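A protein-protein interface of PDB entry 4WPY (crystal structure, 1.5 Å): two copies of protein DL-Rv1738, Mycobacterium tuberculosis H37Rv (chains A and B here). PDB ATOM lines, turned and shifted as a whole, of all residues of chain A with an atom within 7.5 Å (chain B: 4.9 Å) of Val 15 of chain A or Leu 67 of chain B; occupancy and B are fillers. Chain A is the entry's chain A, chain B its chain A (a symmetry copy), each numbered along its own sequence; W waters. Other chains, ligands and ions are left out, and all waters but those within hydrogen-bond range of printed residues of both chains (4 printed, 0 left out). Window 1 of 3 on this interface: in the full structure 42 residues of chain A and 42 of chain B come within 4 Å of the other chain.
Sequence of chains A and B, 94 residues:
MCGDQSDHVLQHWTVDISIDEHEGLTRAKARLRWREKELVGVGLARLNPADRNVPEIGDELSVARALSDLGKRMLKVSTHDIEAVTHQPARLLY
Trp 13 of chain A touches Ile 17 of chain B, and with the chains exchanged Ile 17 of chain A touches Trp 13 of chain B. Thr 14 of chain A touches Val 15 of chain B, and with the chains exchanged Val 15 of chain A touches Thr 14 of chain B. Val 15 of chain A touches its own counterpart, Val 15 of chain B. Ala 64 of chain A touches Gly 71 of chain B, and with the chains exchanged Gly 71 of chain A touches Ala 64 of chain B. Of the 27 pairs that touch across the chains among the printed residues, 21 have their exchanged pair printed and touching as well.
The backbone carbonyl oxygen (O) of Trp 13 of chain A sits at hydrogen-bond distance from the backbone NH (N) of Ile 17 of chain B (2.8 Å). N of Ile 17 of chain A sits at hydrogen-bond distance from O of Trp 13 of chain B (2.8 Å). A ring nitrogen (ND1) of His 12 of chain A sits close to the backbone carbonyl oxygen (O) of Ile 17 of chain B (3.5 Å). The backbone carbonyl oxygen of Val 15 of chain B sits at hydrogen-bond distance from the backbone NH of Val 15 of chain A (3.0 Å).
O of Asp 16 of chain A is in hydrogen-bond range of N of Arg 31 of chain A, at 2.8 Å. The backbone carbonyl oxygen of Ala 64 of chain B lies within hydrogen-bond range of the side-chain hydroxyl of Ser 68 of chain B (3.0 Å). The backbone carbonyl oxygen (O) of Ala 64 of chain A is in hydrogen-bond range of the side-chain hydroxyl (OG) of Ser 68 of chain A, at 3.0 Å.
Water W1 lies within hydrogen-bond range of OG of Ser 68 of chain B, O of Ala 64 of chain B and O of Gly 71 of chain A. Water W4 lies within hydrogen-bond range of the side-chain hydroxyl (OG) of Ser 68 of chain A (2.4 Å), the backbone carbonyl oxygen (O) of Ala 64 of chain A (3.1 Å) and the backbone carbonyl oxygen (O) of Gly 71 of chain B (3.4 Å). Water W3 bridges O of Ser 68 of chain A (2.8 Å) and OG of Ser 68 of chain B (3.1 Å). Water W2 bridges O of Ser 68 of chain B and OG of Ser 68 of chain A.
Of the printed residues of chain B, Val 15 of chain A touches Trp 13 (3.9 Å), Thr 14 (3.3 Å), Val 15 (3.0 Å), Ile 17 (3.6 Å) and Leu 67 (3.96 Å). Printed residues of chain A within 4 Å of Leu 67 of chain B: Val 15 (3.96 Å), Leu 67 (3.9 Å), Leu 70 (3.8 Å) and Met 74 (3.7 Å). No residue of chain A comes within 4 Å of Ala 66 of chain B. Of the printed residues of chain B, Leu 67 of chain A touches Val 15, Leu 67 and Leu 70. Printed residues of chain B within 4 Å of Ser 68 of chain A: Gly 71. Of the printed residues of chain B, Val 63 of chain A touches Trp 13 (3.8 Å). Printed residues of chain A within 4 Å of Ser 68 of chain B: Gly 71 and Lys 72. Ala 30 of chain B touches none of the printed residues of chain A. Ser 18 of chain A touches none of the printed residues of chain B. The nearest printed residue of chain B that does not touch Val 15 of chain A is Val 63 of chain B (6.2 Å). The nearest printed residue of chain B that does not touch Thr 14 of chain A is Ile 17 of chain B (4.8 Å).
Val 15 of chain A touches Thr 14 of chain B (O to CA, 3.3 Å). Val 15 of chain A touches Ile 17 of chain B. Asp 16 of chain A touches Trp 13 of chain B. Ile 17 of chain A touches Val 15 of chain B. Val 63 of chain A touches Trp 13 of chain B (CG2 to CZ3, 3.8 Å). O of Leu 67 of chain B touches O of Leu 67 of chain A (3.9 Å). Gly 71 of chain A touches Ala 64 of chain B (CA to O, 3.7 Å). Gly 71 of chain A touches Ser 68 of chain B. Met 74 of chain A touches Val 63 of chain B (CE to CG1, 3.8 Å). Ala 64 of chain B touches Met 74 of chain A (CB to CB, 3.5 Å).
Of the 14 printed residues of chain B, 10 touch a printed residue of chain A. Printed residues of chain B that touch a printed residue of chain A: Trp 13, Thr 14, Val 15, Ile 17, Val 63, Ala 64, Leu 67, Ser 68, Leu 70 and Gly 71. Hydrophobic or aromatic side chains of chain B within 4 Å of the printed part of chain A: Trp 13, Val 15, Ile 17, Val 63, Ala 64, Leu 67 and Leu 70. Among the printed residues, no Asp or Glu carboxylate lies within 4 Å of a Lys or Arg side-chain nitrogen of the other chain.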
ATOM      1  N   HIS A  12      -9.818 -30.235  18.827  1.00  0.00           N
ATOM      2  CA  HIS A  12      -9.293 -30.235  20.179  1.00  0.00           C
ATOM      3  C   HIS A  12      -8.119 -31.200  20.228  1.00  0.00           C
ATOM      4  O   HIS A  12      -8.272 -32.372  19.880  1.00  0.00           O
ATOM      5  CB  HIS A  12     -10.364 -30.652  21.169  1.00  0.00           C
ATOM      6  CG  HIS A  12      -9.903 -30.563  22.578  1.00  0.00           C
ATOM      7  ND1 HIS A  12     -10.175 -29.483  23.391  1.00  0.00           N
ATOM      8  CD2 HIS A  12      -9.124 -31.396  23.299  1.00  0.00           C
ATOM      9  CE1 HIS A  12      -9.599 -29.677  24.566  1.00  0.00           C
ATOM     10  NE2 HIS A  12      -8.940 -30.821  24.523  1.00  0.00           N
ATOM     11  N   TRP A  13      -6.957 -30.705  20.640  1.00  0.00           N
ATOM     12  CA  TRP A  13      -5.762 -31.521  20.820  1.00  0.00           C
ATOM     13  C   TRP A  13      -5.314 -31.461  22.278  1.00  0.00           C
ATOM     14  O   TRP A  13      -5.711 -30.574  23.034  1.00  0.00           O
ATOM     15  CB  TRP A  13      -4.611 -31.048  19.935  1.00  0.00           C
ATOM     16  CG  TRP A  13      -4.850 -31.065  18.459  1.00  0.00           C
ATOM     17  CD1 TRP A  13      -5.959 -31.511  17.784  1.00  0.00           C
ATOM     18  CD2 TRP A  13      -3.943 -30.583  17.464  1.00  0.00           C
ATOM     19  NE1 TRP A  13      -5.777 -31.349  16.429  1.00  0.00           N
ATOM     20  CE2 TRP A  13      -4.554 -30.771  16.209  1.00  0.00           C
ATOM     21  CE3 TRP A  13      -2.679 -29.996  17.519  1.00  0.00           C
ATOM     22  CZ2 TRP A  13      -3.949 -30.379  15.028  1.00  0.00           C
ATOM     23  CZ3 TRP A  13      -2.078 -29.618  16.355  1.00  0.00           C
ATOM     24  CH2 TRP A  13      -2.707 -29.816  15.118  1.00  0.00           C
ATOM     25  N   THR A  14      -4.433 -32.399  22.651  1.00  0.00           N
ATOM     26  CA  THR A  14      -3.903 -32.536  24.000  1.00  0.00           C
ATOM     27  C   THR A  14      -2.387 -32.651  23.975  1.00  0.00           C
ATOM     28  O   THR A  14      -1.846 -33.431  23.172  1.00  0.00           O
ATOM     29  CB  THR A  14      -4.450 -33.791  24.671  1.00  0.00           C
ATOM     30  OG1 THR A  14      -5.872 -33.799  24.597  1.00  0.00           O
ATOM     31  CG2 THR A  14      -4.027 -33.857  26.099  1.00  0.00           C
ATOM     32  N   VAL A  15      -1.707 -31.938  24.888  1.00  0.00           N
ATOM     33  CA  VAL A  15      -0.290 -32.165  25.157  1.00  0.00           C
ATOM     34  C   VAL A  15      -0.196 -32.949  26.446  1.00  0.00           C
ATOM     35  O   VAL A  15      -0.779 -32.547  27.466  1.00  0.00           O
ATOM     36  CB  VAL A  15       0.503 -30.861  25.284  1.00  0.00           C
ATOM     37  CG1 VAL A  15       1.965 -31.156  25.547  1.00  0.00           C
ATOM     38  CG2 VAL A  15       0.319 -29.987  24.099  1.00  0.00           C
ATOM     39  N   ASP A  16       0.571 -34.037  26.430  1.00  0.00           N
ATOM     40  CA  ASP A  16       0.833 -34.829  27.624  1.00  0.00           C
ATOM     41  C   ASP A  16       2.179 -34.439  28.207  1.00  0.00           C
ATOM     42  O   ASP A  16       3.190 -34.483  27.508  1.00  0.00           O
ATOM     43  CB  ASP A  16       0.831 -36.318  27.289  1.00  0.00           C
ATOM     44  CG  ASP A  16      -0.542 -36.838  26.943  1.00  0.00           C
ATOM     45  OD1 ASP A  16      -1.488 -36.537  27.682  1.00  0.00           O
ATOM     46  OD2 ASP A  16      -0.677 -37.571  25.946  1.00  0.00           O
ATOM     47  N   ILE A  17       2.204 -34.105  29.494  1.00  0.00           N
ATOM     48  CA  ILE A  17       3.413 -33.618  30.144  1.00  0.00           C
ATOM     49  C   ILE A  17       3.783 -34.572  31.272  1.00  0.00           C
ATOM     50  O   ILE A  17       2.976 -34.802  32.178  1.00  0.00           O
ATOM     51  CB  ILE A  17       3.228 -32.196  30.693  1.00  0.00           C
ATOM     52  CG1 ILE A  17       2.697 -31.232  29.630  1.00  0.00           C
ATOM     53  CG2 ILE A  17       4.543 -31.707  31.268  1.00  0.00           C
ATOM     54  CD1 ILE A  17       2.256 -29.876  30.175  1.00  0.00           C
ATOM     55  N   SER A  18       5.015 -35.087  31.248  1.00  0.00           N
ATOM     56  CA  SER A  18       5.565 -35.810  32.390  1.00  0.00           C
ATOM     57  C   SER A  18       6.487 -34.881  33.165  1.00  0.00           C
ATOM     58  O   SER A  18       7.192 -34.063  32.576  1.00  0.00           O
ATOM     59  CB  SER A  18       6.337 -37.064  31.968  1.00  0.00           C
ATOM     60  OG  SER A  18       7.479 -36.695  31.220  1.00  0.00           O
ATOM     61  N   LYS A  29       8.754 -33.386  30.193  1.00  0.00           N
ATOM     62  CA  LYS A  29       8.661 -33.773  28.785  1.00  0.00           C
ATOM     63  C   LYS A  29       7.229 -33.575  28.338  1.00  0.00           C
ATOM     64  O   LYS A  29       6.307 -34.079  28.982  1.00  0.00           O
ATOM     65  CB  LYS A  29       9.109 -35.226  28.588  1.00  0.00           C
ATOM     66  CG  LYS A  29      10.575 -35.407  28.917  1.00  0.00           C
ATOM     67  CD  LYS A  29      11.105 -36.799  28.568  1.00  0.00           C
ATOM     68  CE  LYS A  29      12.586 -36.942  28.898  1.00  0.00           C
ATOM     69  NZ  LYS A  29      13.104 -38.285  28.464  1.00  0.00           N
ATOM     70  N   ALA A  30       7.047 -32.831  27.249  1.00  0.00           N
ATOM     71  CA  ALA A  30       5.731 -32.448  26.748  1.00  0.00           C
ATOM     72  C   ALA A  30       5.562 -33.039  25.354  1.00  0.00           C
ATOM     73  O   ALA A  30       6.177 -32.570  24.399  1.00  0.00           O
ATOM     74  CB  ALA A  30       5.593 -30.934  26.706  1.00  0.00           C
ATOM     75  N   ARG A  31       4.708 -34.037  25.242  1.00  0.00           N
ATOM     76  CA  ARG A  31       4.495 -34.764  23.996  1.00  0.00           C
ATOM     77  C   ARG A  31       3.214 -34.311  23.308  1.00  0.00           C
ATOM     78  O   ARG A  31       2.152 -34.240  23.937  1.00  0.00           O
ATOM     79  CB  ARG A  31       4.419 -36.259  24.267  1.00  0.00           C
ATOM     80  CG  ARG A  31       4.386 -37.105  22.996  1.00  0.00           C
ATOM     81  CD  ARG A  31       4.265 -38.597  23.307  1.00  0.00           C
ATOM     82  NE  ARG A  31       5.314 -39.062  24.201  1.00  0.00           N
ATOM     83  CZ  ARG A  31       6.470 -39.611  23.826  1.00  0.00           C
ATOM     84  NH1 ARG A  31       6.767 -39.792  22.545  1.00  0.00           N
ATOM     85  NH2 ARG A  31       7.339 -39.990  24.755  1.00  0.00           N
ATOM     86  N   LEU A  32       3.307 -34.025  22.018  1.00  0.00           N
ATOM     87  CA  LEU A  32       2.143 -33.734  21.199  1.00  0.00           C
ATOM     88  C   LEU A  32       2.194 -34.587  19.944  1.00  0.00           C
ATOM     89  O   LEU A  32       3.207 -34.600  19.239  1.00  0.00           O
ATOM     90  CB  LEU A  32       2.079 -32.260  20.800  1.00  0.00           C
ATOM     91  CG  LEU A  32       0.952 -31.886  19.857  1.00  0.00           C
ATOM     92  CD1 LEU A  32      -0.414 -32.107  20.480  1.00  0.00           C
ATOM     93  CD2 LEU A  32       1.108 -30.437  19.462  1.00  0.00           C
ATOM     94  N   ARG A  33       1.106 -35.286  19.671  1.00  0.00           N
ATOM     95  CA  ARG A  33       0.907 -36.000  18.418  1.00  0.00           C
ATOM     96  C   ARG A  33      -0.206 -35.310  17.649  1.00  0.00           C
ATOM     97  O   ARG A  33      -1.223 -34.940  18.239  1.00  0.00           O
ATOM     98  CB  ARG A  33       0.490 -37.451  18.657  1.00  0.00           C
ATOM     99  CG  ARG A  33       1.208 -38.148  19.756  1.00  0.00           C
ATOM    100  CD  ARG A  33       0.431 -39.395  20.161  1.00  0.00           C
ATOM    101  NE  ARG A  33       0.354 -40.334  19.064  1.00  0.00           N
ATOM    102  CZ  ARG A  33      -0.475 -41.372  19.021  1.00  0.00           C
ATOM    103  NH1 ARG A  33      -1.333 -41.576  20.022  1.00  0.00           N
ATOM    104  NH2 ARG A  33      -0.433 -42.195  17.969  1.00  0.00           N
ATOM    105  N   LEU A  39       6.057 -34.860  18.425  1.00  0.00           N
ATOM    106  CA  LEU A  39       7.153 -34.111  19.002  1.00  0.00           C
ATOM    107  C   LEU A  39       7.148 -34.268  20.506  1.00  0.00           C
ATOM    108  O   LEU A  39       6.089 -34.422  21.116  1.00  0.00           O
ATOM    109  CB  LEU A  39       7.072 -32.635  18.694  1.00  0.00           C
ATOM    110  CG  LEU A  39       7.206 -32.227  17.254  1.00  0.00           C
ATOM    111  CD1 LEU A  39       6.841 -30.753  17.106  1.00  0.00           C
ATOM    112  CD2 LEU A  39       8.604 -32.510  16.746  1.00  0.00           C
ATOM    113  N   GLY A  41       8.747 -31.878  23.605  1.00  0.00           N
ATOM    114  CA  GLY A  41       9.542 -30.809  24.148  1.00  0.00           C
ATOM    115  C   GLY A  41      10.076 -31.209  25.518  1.00  0.00           C
ATOM    116  O   GLY A  41       9.431 -31.936  26.260  1.00  0.00           O
ATOM    117  N   VAL A  63       8.245 -27.333  33.189  1.00  0.00           N
ATOM    118  CA  VAL A  63       7.152 -27.443  32.227  1.00  0.00           C
ATOM    119  C   VAL A  63       7.106 -26.236  31.292  1.00  0.00           C
ATOM    120  O   VAL A  63       6.897 -26.384  30.081  1.00  0.00           O
ATOM    121  CB  VAL A  63       5.822 -27.647  32.958  1.00  0.00           C
ATOM    122  CG1 VAL A  63       4.632 -27.489  32.000  1.00  0.00           C
ATOM    123  CG2 VAL A  63       5.829 -28.988  33.647  1.00  0.00           C
ATOM    124  N   ALA A  64       7.307 -25.030  31.819  1.00  0.00           N
ATOM    125  CA  ALA A  64       7.370 -23.862  30.953  1.00  0.00           C
ATOM    126  C   ALA A  64       8.396 -24.076  29.865  1.00  0.00           C
ATOM    127  O   ALA A  64       8.165 -23.775  28.688  1.00  0.00           O
ATOM    128  CB  ALA A  64       7.719 -22.628  31.770  1.00  0.00           C
ATOM    129  N   ALA A  66       9.653 -27.012  28.782  1.00  0.00           N
ATOM    130  CA  ALA A  66       9.249 -28.074  27.878  1.00  0.00           C
ATOM    131  C   ALA A  66       8.222 -27.576  26.851  1.00  0.00           C
ATOM    132  O   ALA A  66       8.279 -27.961  25.681  1.00  0.00           O
ATOM    133  CB  ALA A  66       8.698 -29.239  28.683  1.00  0.00           C
ATOM    134  N   LEU A  67       7.279 -26.733  27.271  1.00  0.00           N
ATOM    135  CA  LEU A  67       6.257 -26.230  26.359  1.00  0.00           C
ATOM    136  C   LEU A  67       6.858 -25.254  25.373  1.00  0.00           C
ATOM    137  O   LEU A  67       6.503 -25.248  24.186  1.00  0.00           O
ATOM    138  CB  LEU A  67       5.124 -25.572  27.140  1.00  0.00           C
ATOM    139  CG  LEU A  67       4.289 -26.566  27.916  1.00  0.00           C
ATOM    140  CD1 LEU A  67       3.327 -25.840  28.844  1.00  0.00           C
ATOM    141  CD2 LEU A  67       3.547 -27.516  26.992  1.00  0.00           C
ATOM    142  N   SER A  68       7.778 -24.422  25.839  1.00  0.00           N
ATOM    143  CA  SER A  68       8.473 -23.540  24.926  1.00  0.00           C
ATOM    144  C   SER A  68       9.277 -24.342  23.911  1.00  0.00           C
ATOM    145  O   SER A  68       9.296 -24.008  22.718  1.00  0.00           O
ATOM    146  CB  SER A  68       9.363 -22.591  25.710  1.00  0.00           C
ATOM    147  OG  SER A  68       8.587 -21.759  26.544  1.00  0.00           O
ATOM    148  N   ASP A  69       9.939 -25.410  24.363  1.00  0.00           N
ATOM    149  CA  ASP A  69      10.697 -26.272  23.465  1.00  0.00           C
ATOM    150  C   ASP A  69       9.772 -26.940  22.464  1.00  0.00           C
ATOM    151  O   ASP A  69      10.081 -27.042  21.265  1.00  0.00           O
ATOM    152  CB  ASP A  69      11.452 -27.317  24.301  1.00  0.00           C
ATOM    153  CG  ASP A  69      12.443 -28.135  23.490  1.00  0.00           C
ATOM    154  OD1 ASP A  69      13.270 -27.520  22.794  1.00  0.00           O
ATOM    155  OD2 ASP A  69      12.426 -29.385  23.583  1.00  0.00           O
ATOM    156  N   LEU A  70       8.621 -27.401  22.934  1.00  0.00           N
ATOM    157  CA  LEU A  70       7.660 -28.017  22.033  1.00  0.00           C
ATOM    158  C   LEU A  70       7.186 -27.034  20.967  1.00  0.00           C
ATOM    159  O   LEU A  70       7.137 -27.365  19.771  1.00  0.00           O
ATOM    160  CB  LEU A  70       6.496 -28.566  22.839  1.00  0.00           C
ATOM    161  CG  LEU A  70       5.355 -29.180  22.027  1.00  0.00           C
ATOM    162  CD1 LEU A  70       5.791 -30.322  21.089  1.00  0.00           C
ATOM    163  CD2 LEU A  70       4.301 -29.657  22.983  1.00  0.00           C
ATOM    164  N   GLY A  71       6.846 -25.818  21.376  1.00  0.00           N
ATOM    165  CA  GLY A  71       6.395 -24.828  20.410  1.00  0.00           C
ATOM    166  C   GLY A  71       7.467 -24.489  19.390  1.00  0.00           C
ATOM    167  O   GLY A  71       7.193 -24.368  18.192  1.00  0.00           O
ATOM    168  N   LYS A  72       8.714 -24.391  19.844  1.00  0.00           N
ATOM    169  CA  LYS A  72       9.833 -24.161  18.938  1.00  0.00           C
ATOM    170  C   LYS A  72       9.985 -25.309  17.946  1.00  0.00           C
ATOM    171  O   LYS A  72      10.164 -25.092  16.737  1.00  0.00           O
ATOM    172  CB  LYS A  72      11.105 -23.985  19.766  1.00  0.00           C
ATOM    173  CG  LYS A  72      12.348 -23.668  19.002  1.00  0.00           C
ATOM    174  CD  LYS A  72      13.549 -23.494  19.986  1.00  0.00           C
ATOM    175  CE  LYS A  72      14.843 -24.096  19.449  1.00  0.00           C
ATOM    176  NZ  LYS A  72      15.953 -24.098  20.473  1.00  0.00           N
ATOM    177  N   MET A  74       7.666 -27.281  16.952  1.00  0.00           N
ATOM    178  CA  MET A  74       6.499 -27.267  16.077  1.00  0.00           C
ATOM    179  C   MET A  74       6.584 -26.181  15.027  1.00  0.00           C
ATOM    180  O   MET A  74       6.050 -26.339  13.909  1.00  0.00           O
ATOM    181  CB  MET A  74       5.240 -27.059  16.894  1.00  0.00           C
ATOM    182  CG  MET A  74       4.761 -28.243  17.607  1.00  0.00           C
ATOM    183  SD  MET A  74       3.135 -27.837  18.235  1.00  0.00           S
ATOM    184  CE  MET A  74       2.143 -27.999  16.749  1.00  0.00           C
ATOM    185  N   TRP B  13       0.743 -33.864  33.764  1.00  0.00           N
ATOM    186  CA  TRP B  13      -0.171 -32.762  33.489  1.00  0.00           C
ATOM    187  C   TRP B  13      -0.610 -32.812  32.027  1.00  0.00           C
ATOM    188  O   TRP B  13       0.018 -33.463  31.192  1.00  0.00           O
ATOM    189  CB  TRP B  13       0.473 -31.406  33.760  1.00  0.00           C
ATOM    190  CG  TRP B  13       0.942 -31.154  35.158  1.00  0.00           C
ATOM    191  CD1 TRP B  13       0.814 -31.968  36.255  1.00  0.00           C
ATOM    192  CD2 TRP B  13       1.649 -29.993  35.602  1.00  0.00           C
ATOM    193  NE1 TRP B  13       1.384 -31.365  37.353  1.00  0.00           N
ATOM    194  CE2 TRP B  13       1.912 -30.158  36.976  1.00  0.00           C
ATOM    195  CE3 TRP B  13       2.095 -28.836  34.963  1.00  0.00           C
ATOM    196  CZ2 TRP B  13       2.614 -29.219  37.710  1.00  0.00           C
ATOM    197  CZ3 TRP B  13       2.779 -27.906  35.688  1.00  0.00           C
ATOM    198  CH2 TRP B  13       3.028 -28.094  37.055  1.00  0.00           C
ATOM    199  N   THR B  14      -1.678 -32.065  31.718  1.00  0.00           N
ATOM    200  CA  THR B  14      -2.273 -31.994  30.391  1.00  0.00           C
ATOM    201  C   THR B  14      -2.483 -30.548  29.970  1.00  0.00           C
ATOM    202  O   THR B  14      -3.005 -29.748  30.767  1.00  0.00           O
ATOM    203  CB  THR B  14      -3.634 -32.682  30.371  1.00  0.00           C
ATOM    204  OG1 THR B  14      -3.515 -34.003  30.891  1.00  0.00           O
ATOM    205  CG2 THR B  14      -4.178 -32.741  28.986  1.00  0.00           C
ATOM    206  N   VAL B  15      -2.146 -30.226  28.710  1.00  0.00           N
ATOM    207  CA  VAL B  15      -2.548 -28.964  28.095  1.00  0.00           C
ATOM    208  C   VAL B  15      -3.705 -29.263  27.168  1.00  0.00           C
ATOM    209  O   VAL B  15      -3.606 -30.158  26.314  1.00  0.00           O
ATOM    210  CB  VAL B  15      -1.412 -28.303  27.309  1.00  0.00           C
ATOM    211  CG1 VAL B  15      -1.879 -26.994  26.706  1.00  0.00           C
ATOM    212  CG2 VAL B  15      -0.196 -28.126  28.142  1.00  0.00           C
ATOM    213  N   ILE B  17      -5.936 -27.935  24.063  1.00  0.00           N
ATOM    214  CA  ILE B  17      -5.769 -27.020  22.943  1.00  0.00           C
ATOM    215  C   ILE B  17      -7.055 -26.999  22.128  1.00  0.00           C
ATOM    216  O   ILE B  17      -7.501 -28.046  21.649  1.00  0.00           O
ATOM    217  CB  ILE B  17      -4.585 -27.424  22.053  1.00  0.00           C
ATOM    218  CG1 ILE B  17      -3.298 -27.618  22.858  1.00  0.00           C
ATOM    219  CG2 ILE B  17      -4.399 -26.383  20.965  1.00  0.00           C
ATOM    220  CD1 ILE B  17      -2.157 -28.260  22.073  1.00  0.00           C
ATOM    221  N   ALA B  30      -4.367 -22.676  24.119  1.00  0.00           N
ATOM    222  CA  ALA B  30      -3.752 -23.774  24.859  1.00  0.00           C
ATOM    223  C   ALA B  30      -3.857 -23.462  26.347  1.00  0.00           C
ATOM    224  O   ALA B  30      -3.155 -22.588  26.852  1.00  0.00           O
ATOM    225  CB  ALA B  30      -2.297 -23.946  24.451  1.00  0.00           C
ATOM    226  N   VAL B  63      -1.137 -23.662  16.666  1.00  0.00           N
ATOM    227  CA  VAL B  63      -0.858 -24.381  17.906  1.00  0.00           C
ATOM    228  C   VAL B  63       0.584 -24.167  18.365  1.00  0.00           C
ATOM    229  O   VAL B  63       0.842 -23.968  19.560  1.00  0.00           O
ATOM    230  CB  VAL B  63      -1.186 -25.868  17.742  1.00  0.00           C
ATOM    231  CG1 VAL B  63      -0.648 -26.689  18.922  1.00  0.00           C
ATOM    232  CG2 VAL B  63      -2.674 -26.034  17.558  1.00  0.00           C
ATOM    233  N   ALA B  64       1.543 -24.191  17.442  1.00  0.00           N
ATOM    234  CA  ALA B  64       2.917 -23.894  17.817  1.00  0.00           C
ATOM    235  C   ALA B  64       2.986 -22.565  18.531  1.00  0.00           C
ATOM    236  O   ALA B  64       3.660 -22.414  19.557  1.00  0.00           O
ATOM    237  CB  ALA B  64       3.800 -23.873  16.579  1.00  0.00           C
ATOM    238  N   ARG B  65       2.264 -21.584  17.997  1.00  0.00           N
ATOM    239  CA  ARG B  65       2.271 -20.247  18.564  1.00  0.00           C
ATOM    240  C   ARG B  65       1.585 -20.220  19.918  1.00  0.00           C
ATOM    241  O   ARG B  65       2.059 -19.558  20.852  1.00  0.00           O
ATOM    242  CB  ARG B  65       1.604 -19.304  17.565  1.00  0.00           C
ATOM    243  CG  ARG B  65       2.525 -19.009  16.442  1.00  0.00           C
ATOM    244  CD  ARG B  65       1.848 -18.398  15.242  1.00  0.00           C
ATOM    245  NE  ARG B  65       2.843 -17.961  14.301  1.00  0.00           N
ATOM    246  CZ  ARG B  65       2.591 -17.550  13.061  1.00  0.00           C
ATOM    247  NH1 ARG B  65       1.351 -17.526  12.591  1.00  0.00           N
ATOM    248  NH2 ARG B  65       3.598 -17.188  12.291  1.00  0.00           N
ATOM    249  N   ALA B  66       0.463 -20.919  20.047  1.00  0.00           N
ATOM    250  CA  ALA B  66      -0.226 -20.971  21.323  1.00  0.00           C
ATOM    251  C   ALA B  66       0.644 -21.629  22.404  1.00  0.00           C
ATOM    252  O   ALA B  66       0.647 -21.183  23.554  1.00  0.00           O
ATOM    253  CB  ALA B  66      -1.544 -21.709  21.157  1.00  0.00           C
ATOM    254  N   LEU B  67       1.376 -22.686  22.057  1.00  0.00           N
ATOM    255  CA  LEU B  67       2.214 -23.377  23.032  1.00  0.00           C
ATOM    256  C   LEU B  67       3.406 -22.526  23.405  1.00  0.00           C
ATOM    257  O   LEU B  67       3.814 -22.478  24.573  1.00  0.00           O
ATOM    258  CB  LEU B  67       2.670 -24.725  22.482  1.00  0.00           C
ATOM    259  CG  LEU B  67       1.544 -25.729  22.375  1.00  0.00           C
ATOM    260  CD1 LEU B  67       2.005 -26.964  21.618  1.00  0.00           C
ATOM    261  CD2 LEU B  67       0.992 -26.098  23.741  1.00  0.00           C
ATOM    262  N   SER B  68       3.979 -21.837  22.429  1.00  0.00           N
ATOM    263  CA  SER B  68       5.053 -20.917  22.738  1.00  0.00           C
ATOM    264  C   SER B  68       4.559 -19.799  23.648  1.00  0.00           C
ATOM    265  O   SER B  68       5.251 -19.408  24.597  1.00  0.00           O
ATOM    266  CB  SER B  68       5.638 -20.362  21.451  1.00  0.00           C
ATOM    267  OG  SER B  68       6.217 -21.396  20.684  1.00  0.00           O
ATOM    268  N   ASP B  69       3.358 -19.280  23.379  1.00  0.00           N
ATOM    269  CA  ASP B  69       2.773 -18.242  24.218  1.00  0.00           C
ATOM    270  C   ASP B  69       2.525 -18.769  25.620  1.00  0.00           C
ATOM    271  O   ASP B  69       2.786 -18.086  26.624  1.00  0.00           O
ATOM    272  CB  ASP B  69       1.466 -17.759  23.571  1.00  0.00           C
ATOM    273  CG  ASP B  69       0.878 -16.530  24.244  1.00  0.00           C
ATOM    274  OD1 ASP B  69       1.621 -15.546  24.405  1.00  0.00           O
ATOM    275  OD2 ASP B  69      -0.333 -16.531  24.570  1.00  0.00           O
ATOM    276  N   LEU B  70       2.022 -19.992  25.715  1.00  0.00           N
ATOM    277  CA  LEU B  70       1.795 -20.588  27.021  1.00  0.00           C
ATOM    278  C   LEU B  70       3.096 -20.728  27.805  1.00  0.00           C
ATOM    279  O   LEU B  70       3.165 -20.376  28.994  1.00  0.00           O
ATOM    280  CB  LEU B  70       1.103 -21.929  26.849  1.00  0.00           C
ATOM    281  CG  LEU B  70       0.862 -22.723  28.133  1.00  0.00           C
ATOM    282  CD1 LEU B  70       0.048 -21.967  29.200  1.00  0.00           C
ATOM    283  CD2 LEU B  70       0.183 -24.012  27.769  1.00  0.00           C
ATOM    284  N   GLY B  71       4.140 -21.226  27.156  1.00  0.00           N
ATOM    285  CA  GLY B  71       5.415 -21.377  27.840  1.00  0.00           C
ATOM    286  C   GLY B  71       5.982 -20.045  28.300  1.00  0.00           C
ATOM    287  O   GLY B  71       6.497 -19.923  29.417  1.00  0.00           O
HETATM  288  O   HOH W   1       6.200 -21.115  18.256  1.00  0.00           O
HETATM  289  O   HOH W   2       8.011 -19.669  24.384  1.00  0.00           O
HETATM  290  O   HOH W   3       8.919 -21.319  22.118  1.00  0.00           O
HETATM  291  O   HOH W   4       9.623 -21.001  28.624  1.00  0.00           O
